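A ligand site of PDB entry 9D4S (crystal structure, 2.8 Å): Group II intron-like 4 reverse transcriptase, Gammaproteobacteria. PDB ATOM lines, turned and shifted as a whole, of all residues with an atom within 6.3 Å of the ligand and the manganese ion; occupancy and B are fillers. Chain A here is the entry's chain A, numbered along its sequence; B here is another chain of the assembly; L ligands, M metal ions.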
ATOM      1  N   LYS A  71     -13.630  25.925  -6.331  1.00  0.00           N
ATOM      2  CA  LYS A  71     -15.002  25.365  -6.303  1.00  0.00           C
ATOM      3  C   LYS A  71     -14.835  23.853  -6.125  1.00  0.00           C
ATOM      4  O   LYS A  71     -13.744  23.344  -6.403  1.00  0.00           O
ATOM      5  CB  LYS A  71     -15.761  25.682  -7.594  1.00  0.00           C
ATOM      6  CG  LYS A  71     -16.681  26.885  -7.554  1.00  0.00           C
ATOM      7  CD  LYS A  71     -17.330  27.106  -8.887  1.00  0.00           C
ATOM      8  CE  LYS A  71     -17.857  25.835  -9.513  1.00  0.00           C
ATOM      9  NZ  LYS A  71     -18.507  26.087 -10.825  1.00  0.00           N
ATOM     10  N   LYS A  75     -13.282  22.691 -10.900  1.00  0.00           N
ATOM     11  CA  LYS A  75     -13.894  23.902 -11.494  1.00  0.00           C
ATOM     12  C   LYS A  75     -13.568  25.155 -10.677  1.00  0.00           C
ATOM     13  O   LYS A  75     -13.283  25.013  -9.486  1.00  0.00           O
ATOM     14  CB  LYS A  75     -15.404  23.651 -11.566  1.00  0.00           C
ATOM     15  CG  LYS A  75     -15.816  22.280 -12.083  1.00  0.00           C
ATOM     16  CD  LYS A  75     -17.303  22.034 -11.993  1.00  0.00           C
ATOM     17  CE  LYS A  75     -17.708  20.691 -12.554  1.00  0.00           C
ATOM     18  NZ  LYS A  75     -19.158  20.456 -12.439  1.00  0.00           N
ATOM     19  N   ARG A  77     -14.958  29.336 -10.000  1.00  0.00           N
ATOM     20  CA  ARG A  77     -15.962  30.357 -10.294  1.00  0.00           C
ATOM     21  C   ARG A  77     -15.204  31.607 -10.763  1.00  0.00           C
ATOM     22  O   ARG A  77     -14.393  32.136  -9.999  1.00  0.00           O
ATOM     23  CB  ARG A  77     -16.847  30.657  -9.074  1.00  0.00           C
ATOM     24  CG  ARG A  77     -18.189  31.344  -9.418  1.00  0.00           C
ATOM     25  CD  ARG A  77     -19.373  31.189  -8.379  1.00  0.00           C
ATOM     26  NE  ARG A  77     -19.876  29.823  -8.143  1.00  0.00           N
ATOM     27  CZ  ARG A  77     -20.319  28.970  -9.073  1.00  0.00           C
ATOM     28  NH1 ARG A  77     -20.406  29.314 -10.355  1.00  0.00           N
ATOM     29  NH2 ARG A  77     -20.668  27.733  -8.713  1.00  0.00           N
ATOM     30  N   ASP A 144     -28.290  19.812 -16.570  1.00  0.00           N
ATOM     31  CA  ASP A 144     -27.721  21.154 -16.246  1.00  0.00           C
ATOM     32  C   ASP A 144     -26.834  21.575 -17.429  1.00  0.00           C
ATOM     33  O   ASP A 144     -26.395  20.692 -18.151  1.00  0.00           O
ATOM     34  CB  ASP A 144     -26.932  21.080 -14.931  1.00  0.00           C
ATOM     35  CG  ASP A 144     -26.299  22.362 -14.443  1.00  0.00           C
ATOM     36  OD1 ASP A 144     -25.320  22.804 -15.055  1.00  0.00           O
ATOM     37  OD2 ASP A 144     -26.760  22.888 -13.421  1.00  0.00           O
ATOM     38  N   ILE A 145     -26.590  22.875 -17.579  1.00  0.00           N
ATOM     39  CA  ILE A 145     -25.678  23.361 -18.648  1.00  0.00           C
ATOM     40  C   ILE A 145     -24.297  23.563 -18.040  1.00  0.00           C
ATOM     41  O   ILE A 145     -24.192  24.251 -17.016  1.00  0.00           O
ATOM     42  CB  ILE A 145     -26.206  24.696 -19.218  1.00  0.00           C
ATOM     43  CG1 ILE A 145     -27.623  24.557 -19.780  1.00  0.00           C
ATOM     44  CG2 ILE A 145     -25.245  25.255 -20.253  1.00  0.00           C
ATOM     45  CD1 ILE A 145     -28.192  25.861 -20.286  1.00  0.00           C
ATOM     46  N   PRO A 146     -23.234  22.955 -18.601  1.00  0.00           N
ATOM     47  CA  PRO A 146     -21.882  23.187 -18.120  1.00  0.00           C
ATOM     48  C   PRO A 146     -21.363  24.613 -18.359  1.00  0.00           C
ATOM     49  O   PRO A 146     -21.516  25.077 -19.459  1.00  0.00           O
ATOM     50  CB  PRO A 146     -21.049  22.282 -19.024  1.00  0.00           C
ATOM     51  CG  PRO A 146     -21.982  21.218 -19.526  1.00  0.00           C
ATOM     52  CD  PRO A 146     -23.297  21.944 -19.654  1.00  0.00           C
ATOM     53  N   ALA A 147     -20.765  25.243 -17.349  1.00  0.00           N
ATOM     54  CA  ALA A 147     -20.122  26.566 -17.546  1.00  0.00           C
ATOM     55  C   ALA A 147     -21.106  27.522 -18.218  1.00  0.00           C
ATOM     56  O   ALA A 147     -20.685  28.204 -19.150  1.00  0.00           O
ATOM     57  CB  ALA A 147     -18.858  26.402 -18.324  1.00  0.00           C
ATOM     58  N   PHE A 148     -22.342  27.595 -17.745  1.00  0.00           N
ATOM     59  CA  PHE A 148     -23.362  28.358 -18.505  1.00  0.00           C
ATOM     60  C   PHE A 148     -23.009  29.844 -18.665  1.00  0.00           C
ATOM     61  O   PHE A 148     -23.089  30.318 -19.796  1.00  0.00           O
ATOM     62  CB  PHE A 148     -24.696  28.149 -17.797  1.00  0.00           C
ATOM     63  CG  PHE A 148     -25.880  28.913 -18.319  1.00  0.00           C
ATOM     64  CD1 PHE A 148     -26.080  29.079 -19.682  1.00  0.00           C
ATOM     65  CD2 PHE A 148     -26.826  29.414 -17.444  1.00  0.00           C
ATOM     66  CE1 PHE A 148     -27.173  29.780 -20.153  1.00  0.00           C
ATOM     67  CE2 PHE A 148     -27.929  30.101 -17.914  1.00  0.00           C
ATOM     68  CZ  PHE A 148     -28.093  30.291 -19.272  1.00  0.00           C
ATOM     69  N   PHE A 149     -22.553  30.514 -17.615  1.00  0.00           N
ATOM     70  CA  PHE A 149     -22.276  31.971 -17.706  1.00  0.00           C
ATOM     71  C   PHE A 149     -21.129  32.219 -18.678  1.00  0.00           C
ATOM     72  O   PHE A 149     -21.152  33.211 -19.398  1.00  0.00           O
ATOM     73  CB  PHE A 149     -22.171  32.596 -16.307  1.00  0.00           C
ATOM     74  CG  PHE A 149     -23.508  32.941 -15.694  1.00  0.00           C
ATOM     75  CD1 PHE A 149     -24.651  32.222 -16.013  1.00  0.00           C
ATOM     76  CD2 PHE A 149     -23.618  33.993 -14.799  1.00  0.00           C
ATOM     77  CE1 PHE A 149     -25.873  32.539 -15.444  1.00  0.00           C
ATOM     78  CE2 PHE A 149     -24.853  34.305 -14.233  1.00  0.00           C
ATOM     79  CZ  PHE A 149     -25.967  33.579 -14.563  1.00  0.00           C
ATOM     80  N   THR A 150     -20.128  31.346 -18.654  1.00  0.00           N
ATOM     81  CA  THR A 150     -18.942  31.441 -19.535  1.00  0.00           C
ATOM     82  C   THR A 150     -19.327  31.337 -21.015  1.00  0.00           C
ATOM     83  O   THR A 150     -18.641  31.954 -21.836  1.00  0.00           O
ATOM     84  CB  THR A 150     -17.933  30.355 -19.182  1.00  0.00           C
ATOM     85  OG1 THR A 150     -18.353  29.148 -19.812  1.00  0.00           O
ATOM     86  CG2 THR A 150     -17.793  30.145 -17.688  1.00  0.00           C
ATOM     87  N   GLN A 206     -19.595  37.011 -13.678  1.00  0.00           N
ATOM     88  CA  GLN A 206     -20.204  36.426 -12.474  1.00  0.00           C
ATOM     89  C   GLN A 206     -19.929  37.456 -11.392  1.00  0.00           C
ATOM     90  O   GLN A 206     -18.755  37.797 -11.231  1.00  0.00           O
ATOM     91  CB  GLN A 206     -19.679  35.013 -12.263  1.00  0.00           C
ATOM     92  CG  GLN A 206     -20.358  34.018 -13.202  1.00  0.00           C
ATOM     93  CD  GLN A 206     -19.769  32.634 -13.218  1.00  0.00           C
ATOM     94  OE1 GLN A 206     -19.745  31.924 -12.215  1.00  0.00           O
ATOM     95  NE2 GLN A 206     -19.296  32.221 -14.385  1.00  0.00           N
ATOM     96  N   GLY A 207     -20.920  37.823 -10.594  1.00  0.00           N
ATOM     97  CA  GLY A 207     -20.787  38.977  -9.683  1.00  0.00           C
ATOM     98  C   GLY A 207     -21.451  40.211 -10.263  1.00  0.00           C
ATOM     99  O   GLY A 207     -21.380  41.264  -9.616  1.00  0.00           O
ATOM    100  N   PRO A 212     -27.722  37.171 -14.159  1.00  0.00           N
ATOM    101  CA  PRO A 212     -28.795  36.184 -14.024  1.00  0.00           C
ATOM    102  C   PRO A 212     -29.999  36.468 -14.948  1.00  0.00           C
ATOM    103  O   PRO A 212     -30.500  35.524 -15.505  1.00  0.00           O
ATOM    104  CB  PRO A 212     -29.164  36.328 -12.547  1.00  0.00           C
ATOM    105  CG  PRO A 212     -27.869  36.708 -11.905  1.00  0.00           C
ATOM    106  CD  PRO A 212     -27.318  37.731 -12.869  1.00  0.00           C
ATOM    107  N   ILE A 237     -32.545  28.800 -13.513  1.00  0.00           N
ATOM    108  CA  ILE A 237     -31.213  29.109 -14.111  1.00  0.00           C
ATOM    109  C   ILE A 237     -30.940  28.026 -15.151  1.00  0.00           C
ATOM    110  O   ILE A 237     -31.758  27.882 -16.039  1.00  0.00           O
ATOM    111  CB  ILE A 237     -30.100  29.267 -13.047  1.00  0.00           C
ATOM    112  CG1 ILE A 237     -30.604  29.985 -11.794  1.00  0.00           C
ATOM    113  CG2 ILE A 237     -28.890  29.972 -13.625  1.00  0.00           C
ATOM    114  CD1 ILE A 237     -30.515  31.486 -11.886  1.00  0.00           C
ATOM    115  N   ASP A 238     -29.751  27.414 -15.146  1.00  0.00           N
ATOM    116  CA  ASP A 238     -29.391  26.281 -16.039  1.00  0.00           C
ATOM    117  C   ASP A 238     -30.152  24.975 -15.764  1.00  0.00           C
ATOM    118  O   ASP A 238     -30.417  24.263 -16.727  1.00  0.00           O
ATOM    119  CB  ASP A 238     -27.871  26.098 -16.108  1.00  0.00           C
ATOM    120  CG  ASP A 238     -27.163  25.738 -14.830  1.00  0.00           C
ATOM    121  OD1 ASP A 238     -27.818  25.715 -13.777  1.00  0.00           O
ATOM    122  OD2 ASP A 238     -25.958  25.475 -14.915  1.00  0.00           O
ATOM    123  N   ASP A 239     -30.422  24.639 -14.500  1.00  0.00           N
ATOM    124  CA  ASP A 239     -31.008  23.293 -14.206  1.00  0.00           C
ATOM    125  C   ASP A 239     -32.379  23.146 -14.851  1.00  0.00           C
ATOM    126  O   ASP A 239     -33.214  24.036 -14.682  1.00  0.00           O
ATOM    127  CB  ASP A 239     -31.128  23.051 -12.708  1.00  0.00           C
ATOM    128  CG  ASP A 239     -29.829  22.717 -12.008  1.00  0.00           C
ATOM    129  OD1 ASP A 239     -28.943  23.589 -11.980  1.00  0.00           O
ATOM    130  OD2 ASP A 239     -29.711  21.590 -11.503  1.00  0.00           O
ATOM    131  N   TYR A 269     -25.400  18.205 -19.441  1.00  0.00           N
ATOM    132  CA  TYR A 269     -24.785  16.983 -18.905  1.00  0.00           C
ATOM    133  C   TYR A 269     -25.627  15.778 -19.326  1.00  0.00           C
ATOM    134  O   TYR A 269     -26.861  15.880 -19.312  1.00  0.00           O
ATOM    135  CB  TYR A 269     -24.652  17.136 -17.396  1.00  0.00           C
ATOM    136  CG  TYR A 269     -23.534  18.042 -16.954  1.00  0.00           C
ATOM    137  CD1 TYR A 269     -22.222  17.590 -16.977  1.00  0.00           C
ATOM    138  CD2 TYR A 269     -23.768  19.342 -16.548  1.00  0.00           C
ATOM    139  CE1 TYR A 269     -21.179  18.400 -16.580  1.00  0.00           C
ATOM    140  CE2 TYR A 269     -22.733  20.164 -16.142  1.00  0.00           C
ATOM    141  CZ  TYR A 269     -21.431  19.698 -16.165  1.00  0.00           C
ATOM    142  OH  TYR A 269     -20.383  20.482 -15.781  1.00  0.00           O
ATOM    143  N   LYS A 277     -24.849  15.340 -12.286  1.00  0.00           N
ATOM    144  CA  LYS A 277     -25.482  16.558 -12.874  1.00  0.00           C
ATOM    145  C   LYS A 277     -26.724  16.259 -13.717  1.00  0.00           C
ATOM    146  O   LYS A 277     -27.390  17.231 -14.111  1.00  0.00           O
ATOM    147  CB  LYS A 277     -24.408  17.368 -13.617  1.00  0.00           C
ATOM    148  CG  LYS A 277     -23.192  17.742 -12.790  1.00  0.00           C
ATOM    149  CD  LYS A 277     -22.902  19.223 -12.775  1.00  0.00           C
ATOM    150  CE  LYS A 277     -24.072  20.056 -12.271  1.00  0.00           C
ATOM    151  NZ  LYS A 277     -23.685  21.468 -12.054  1.00  0.00           N
ATOM    152  P    DG B   3     -18.041  39.395  -1.323  1.00  0.00           P
ATOM    153  OP1  DG B   3     -18.202  40.644  -0.512  1.00  0.00           O
ATOM    154  OP2  DG B   3     -18.604  38.154  -0.672  1.00  0.00           O
ATOM    155  O5'  DG B   3     -18.866  39.615  -2.663  1.00  0.00           O
ATOM    156  C5'  DG B   3     -18.368  40.598  -3.603  1.00  0.00           C
ATOM    157  C4'  DG B   3     -18.958  40.313  -4.961  1.00  0.00           C
ATOM    158  O4'  DG B   3     -18.420  39.073  -5.473  1.00  0.00           O
ATOM    159  C3'  DG B   3     -20.459  40.101  -4.971  1.00  0.00           C
ATOM    160  O3'  DG B   3     -21.170  41.335  -4.985  1.00  0.00           O
ATOM    161  C2'  DG B   3     -20.631  39.357  -6.281  1.00  0.00           C
ATOM    162  C1'  DG B   3     -19.417  38.456  -6.291  1.00  0.00           C
ATOM    163  N9   DG B   3     -19.698  37.127  -5.765  1.00  0.00           N
ATOM    164  C8   DG B   3     -19.313  36.556  -4.576  1.00  0.00           C
ATOM    165  N7   DG B   3     -19.741  35.331  -4.434  1.00  0.00           N
ATOM    166  C5   DG B   3     -20.439  35.073  -5.612  1.00  0.00           C
ATOM    167  C6   DG B   3     -21.119  33.908  -6.027  1.00  0.00           C
ATOM    168  O6   DG B   3     -21.248  32.836  -5.421  1.00  0.00           O
ATOM    169  N1   DG B   3     -21.692  34.077  -7.295  1.00  0.00           N
ATOM    170  C2   DG B   3     -21.621  35.227  -8.052  1.00  0.00           C
ATOM    171  N2   DG B   3     -22.234  35.208  -9.232  1.00  0.00           N
ATOM    172  N3   DG B   3     -20.970  36.321  -7.658  1.00  0.00           N
ATOM    173  C4   DG B   3     -20.407  36.171  -6.445  1.00  0.00           C
ATOM    174  P    DC B   4     -22.730  41.381  -4.641  1.00  0.00           P
ATOM    175  OP1  DC B   4     -23.211  42.804  -4.692  1.00  0.00           O
ATOM    176  OP2  DC B   4     -23.034  40.671  -3.363  1.00  0.00           O
ATOM    177  O5'  DC B   4     -23.478  40.597  -5.813  1.00  0.00           O
ATOM    178  C5'  DC B   4     -23.523  41.173  -7.134  1.00  0.00           C
ATOM    179  C4'  DC B   4     -24.284  40.258  -8.062  1.00  0.00           C
ATOM    180  O4'  DC B   4     -23.660  38.955  -8.129  1.00  0.00           O
ATOM    181  C3'  DC B   4     -25.690  39.941  -7.597  1.00  0.00           C
ATOM    182  O3'  DC B   4     -26.582  41.018  -7.867  1.00  0.00           O
ATOM    183  C2'  DC B   4     -25.982  38.699  -8.413  1.00  0.00           C
ATOM    184  C1'  DC B   4     -24.648  37.971  -8.331  1.00  0.00           C
ATOM    185  N1   DC B   4     -24.561  37.014  -7.210  1.00  0.00           N
ATOM    186  C2   DC B   4     -25.097  35.740  -7.387  1.00  0.00           C
ATOM    187  O2   DC B   4     -25.661  35.469  -8.452  1.00  0.00           O
ATOM    188  N3   DC B   4     -25.011  34.850  -6.379  1.00  0.00           N
ATOM    189  C4   DC B   4     -24.404  35.180  -5.231  1.00  0.00           C
ATOM    190  N4   DC B   4     -24.347  34.258  -4.279  1.00  0.00           N
ATOM    191  C5   DC B   4     -23.826  36.460  -5.041  1.00  0.00           C
ATOM    192  C6   DC B   4     -23.927  37.332  -6.057  1.00  0.00           C
ATOM    193  P    DC B  17     -29.217  23.801  -1.153  1.00  0.00           P
ATOM    194  OP1  DC B  17     -29.259  22.326  -1.340  1.00  0.00           O
ATOM    195  OP2  DC B  17     -27.942  24.468  -0.812  1.00  0.00           O
ATOM    196  O5'  DC B  17     -29.788  24.531  -2.447  1.00  0.00           O
ATOM    197  C5'  DC B  17     -31.057  24.226  -2.893  1.00  0.00           C
ATOM    198  C4'  DC B  17     -31.426  25.093  -4.054  1.00  0.00           C
ATOM    199  O4'  DC B  17     -31.652  26.437  -3.628  1.00  0.00           O
ATOM    200  C3'  DC B  17     -30.339  25.225  -5.105  1.00  0.00           C
ATOM    201  O3'  DC B  17     -30.392  24.094  -5.933  1.00  0.00           O
ATOM    202  C2'  DC B  17     -30.796  26.480  -5.845  1.00  0.00           C
ATOM    203  C1'  DC B  17     -31.389  27.314  -4.711  1.00  0.00           C
ATOM    204  N1   DC B  17     -30.498  28.386  -4.243  1.00  0.00           N
ATOM    205  C2   DC B  17     -30.547  29.629  -4.875  1.00  0.00           C
ATOM    206  O2   DC B  17     -31.378  29.815  -5.764  1.00  0.00           O
ATOM    207  N3   DC B  17     -29.708  30.609  -4.428  1.00  0.00           N
ATOM    208  C4   DC B  17     -28.874  30.369  -3.421  1.00  0.00           C
ATOM    209  N4   DC B  17     -28.077  31.349  -3.028  1.00  0.00           N
ATOM    210  C5   DC B  17     -28.795  29.083  -2.781  1.00  0.00           C
ATOM    211  C6   DC B  17     -29.609  28.135  -3.221  1.00  0.00           C
ATOM    212  P   DDG B  18     -29.186  23.488  -6.710  1.00  0.00           P
ATOM    213  OP1 DDG B  18     -29.000  22.059  -6.954  1.00  0.00           O
ATOM    214  OP2 DDG B  18     -27.927  24.122  -6.077  1.00  0.00           O
ATOM    215  O5' DDG B  18     -29.570  24.197  -8.141  1.00  0.00           O
ATOM    216  C5' DDG B  18     -28.582  25.033  -8.727  1.00  0.00           C
ATOM    217  C4' DDG B  18     -29.282  26.096  -9.596  1.00  0.00           C
ATOM    218  O4' DDG B  18     -29.612  27.381  -8.791  1.00  0.00           O
ATOM    219  C3' DDG B  18     -28.445  26.451 -10.489  1.00  0.00           C
ATOM    220  C2' DDG B  18     -27.601  27.616  -9.807  1.00  0.00           C
ATOM    221  C1' DDG B  18     -28.471  28.297  -9.098  1.00  0.00           C
ATOM    222  N9  DDG B  18     -27.837  28.671  -7.775  1.00  0.00           N
ATOM    223  C8  DDG B  18     -27.577  27.974  -6.639  1.00  0.00           C
ATOM    224  N7  DDG B  18     -27.001  28.827  -5.780  1.00  0.00           N
ATOM    225  C5  DDG B  18     -26.931  30.013  -6.393  1.00  0.00           C
ATOM    226  C6  DDG B  18     -26.375  31.377  -5.948  1.00  0.00           C
ATOM    227  O6  DDG B  18     -25.893  31.503  -4.822  1.00  0.00           O
ATOM    228  N1  DDG B  18     -26.446  32.467  -6.862  1.00  0.00           N
ATOM    229  C2  DDG B  18     -27.009  32.320  -8.173  1.00  0.00           C
ATOM    230  N2  DDG B  18     -27.059  33.432  -9.047  1.00  0.00           N
ATOM    231  N3  DDG B  18     -27.521  31.047  -8.591  1.00  0.00           N
ATOM    232  C4  DDG B  18     -27.449  29.893  -7.642  1.00  0.00           C
HETATM  233  N1  LIG L   1     -24.190  31.024 -10.298  1.00  0.00           N
HETATM  234  C1  LIG L   1     -23.651  32.151  -9.649  1.00  0.00           C
HETATM  235  N2  LIG L   1     -23.269  32.043  -8.364  1.00  0.00           N
HETATM  236  C2  LIG L   1     -23.406  30.878  -7.704  1.00  0.00           C
HETATM  237  C3  LIG L   1     -23.967  29.718  -8.335  1.00  0.00           C
HETATM  238  C4  LIG L   1     -24.324  29.836  -9.614  1.00  0.00           C
HETATM  239  O1  LIG L   1     -23.536  33.197 -10.283  1.00  0.00           O
HETATM  240  N3  LIG L   1     -22.994  30.826  -6.441  1.00  0.00           N
HETATM  241  C5  LIG L   1     -24.584  31.163 -11.720  1.00  0.00           C
HETATM  242  C6  LIG L   1     -23.397  31.226 -12.685  1.00  0.00           C
HETATM  243  C7  LIG L   1     -23.286  29.792 -13.164  1.00  0.00           C
HETATM  244  C8  LIG L   1     -24.754  29.410 -13.261  1.00  0.00           C
HETATM  245  O2  LIG L   1     -25.346  30.023 -12.093  1.00  0.00           O
HETATM  246  O3  LIG L   1     -22.606  29.688 -14.412  1.00  0.00           O
HETATM  247  C9  LIG L   1     -25.058  27.930 -13.319  1.00  0.00           C
HETATM  248  O4  LIG L   1     -24.809  27.348 -12.027  1.00  0.00           O
HETATM  249  P1  LIG L   1     -24.007  26.010 -11.866  1.00  0.00           P
HETATM  250  O5  LIG L   1     -23.743  25.765 -10.442  1.00  0.00           O
HETATM  251  O6  LIG L   1     -24.742  24.884 -12.614  1.00  0.00           O
HETATM  252  O7  LIG L   1     -22.595  26.321 -12.545  1.00  0.00           O
HETATM  253  P2  LIG L   1     -21.895  26.153 -13.969  1.00  0.00           P
HETATM  254  O8  LIG L   1     -21.020  27.316 -14.186  1.00  0.00           O
HETATM  255  O9  LIG L   1     -22.960  25.917 -15.041  1.00  0.00           O
HETATM  256  O10 LIG L   1     -21.090  24.832 -13.742  1.00  0.00           O
HETATM  257  P3  LIG L   1     -21.209  23.260 -13.973  1.00  0.00           P
HETATM  258  O11 LIG L   1     -20.472  22.889 -15.177  1.00  0.00           O
HETATM  259  O12 LIG L   1     -20.620  22.644 -12.715  1.00  0.00           O
HETATM  260  O13 LIG L   1     -22.728  22.982 -14.025  1.00  0.00           O
HETATM  261 MN    MN M   1     -24.240  24.299 -14.847  1.00  0.00          MN
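O of Asp 144 is in hydrogen-bond range of N of Tyr 269 (3.0 Å).
The side-chain carboxylate of Asp 144 is in salt-bridge range of the side-chain amino group of Lys 277 (3.7 Å).
OD1 of Asp 239 sits close to OD2 of Asp 144 (2.7 Å).
N2 of DG 3 of chain B lies within hydrogen-bond range of N of Gly 207 (3.2 Å).
The backbone carbonyl oxygen (O) of Ala 147 sits at hydrogen-bond distance from the side-chain hydroxyl (OG1) of Thr 150, 2.6 Å away.
N2 of DDG 18 of chain B sits close to O2 of DC 4 of chain B, at 2.5 Å.
OE1 of Gln 206 sits close to NH1 of Arg 77, at 3.3 Å.
The side-chain hydroxyl (OH) of Tyr 269 sits at hydrogen-bond distance from an oxygen (O11) of the ligand, 2.5 Å away.
O6 of DG 3 of chain B sits at hydrogen-bond distance from N3 of the ligand (2.9 Å).
The side-chain amino group of Lys 75 is in salt-bridge range of an oxygen (O12) of the ligand (2.6 Å).
The side-chain amino group (NZ) of Lys 277 lies within salt-bridge range of an oxygen (O12) of the ligand, at 3.3 Å.
An oxygen (O11) of the ligand sits at hydrogen-bond distance from the backbone NH (N) of Ala 147 (3.2 Å).
An oxygen (O9) of the ligand lies close to the backbone NH (N) of Phe 148.
N of Phe 149 is in hydrogen-bond range of O3 of the ligand, at 3.3 Å.
O6 of DDG 18 of chain B lies within hydrogen-bond range of a nitrogen (N3) of the ligand.
NE of Arg 77 touches N3 of the ligand (3.7 Å).
Pro 146 touches the ligand.
OE1 of Gln 206 touches C6 of the ligand, 3.7 Å away.
CG2 of Ile 237 touches O2 of the ligand, 3.9 Å away.
DC 4 of chain B touches the ligand.
Within 4 Å of the ligand: Lys 75, Arg 77, Asp 144, Ile 145, Pro 146, Ala 147, Phe 148, Phe 149, Gln 206, Ile 237, Asp 238, Tyr 269, Lys 277, DG 3 of chain B, DC 4 of chain B and DDG 18 of chain B.
The manganese ion is bound by the side-chain carboxylate (OD1) of Asp 144 (1.9 Å), an oxygen (O9) of the ligand (2.1 Å), the side-chain carboxylate (OD2) of Asp 238 (2.1 Å), an oxygen (O13) of the ligand (2.2 Å), the backbone carbonyl oxygen (O) of Ile 145 (2.2 Å) and an oxygen (O6) of the ligand (2.4 Å).
The manganese ion has six donor atoms within binding distance.
Of the 22 residues printed, 3 come within 4 Å of the manganese ion.
Along chain A the residues within 4 Å of the manganese ion span positions 144 to 238.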
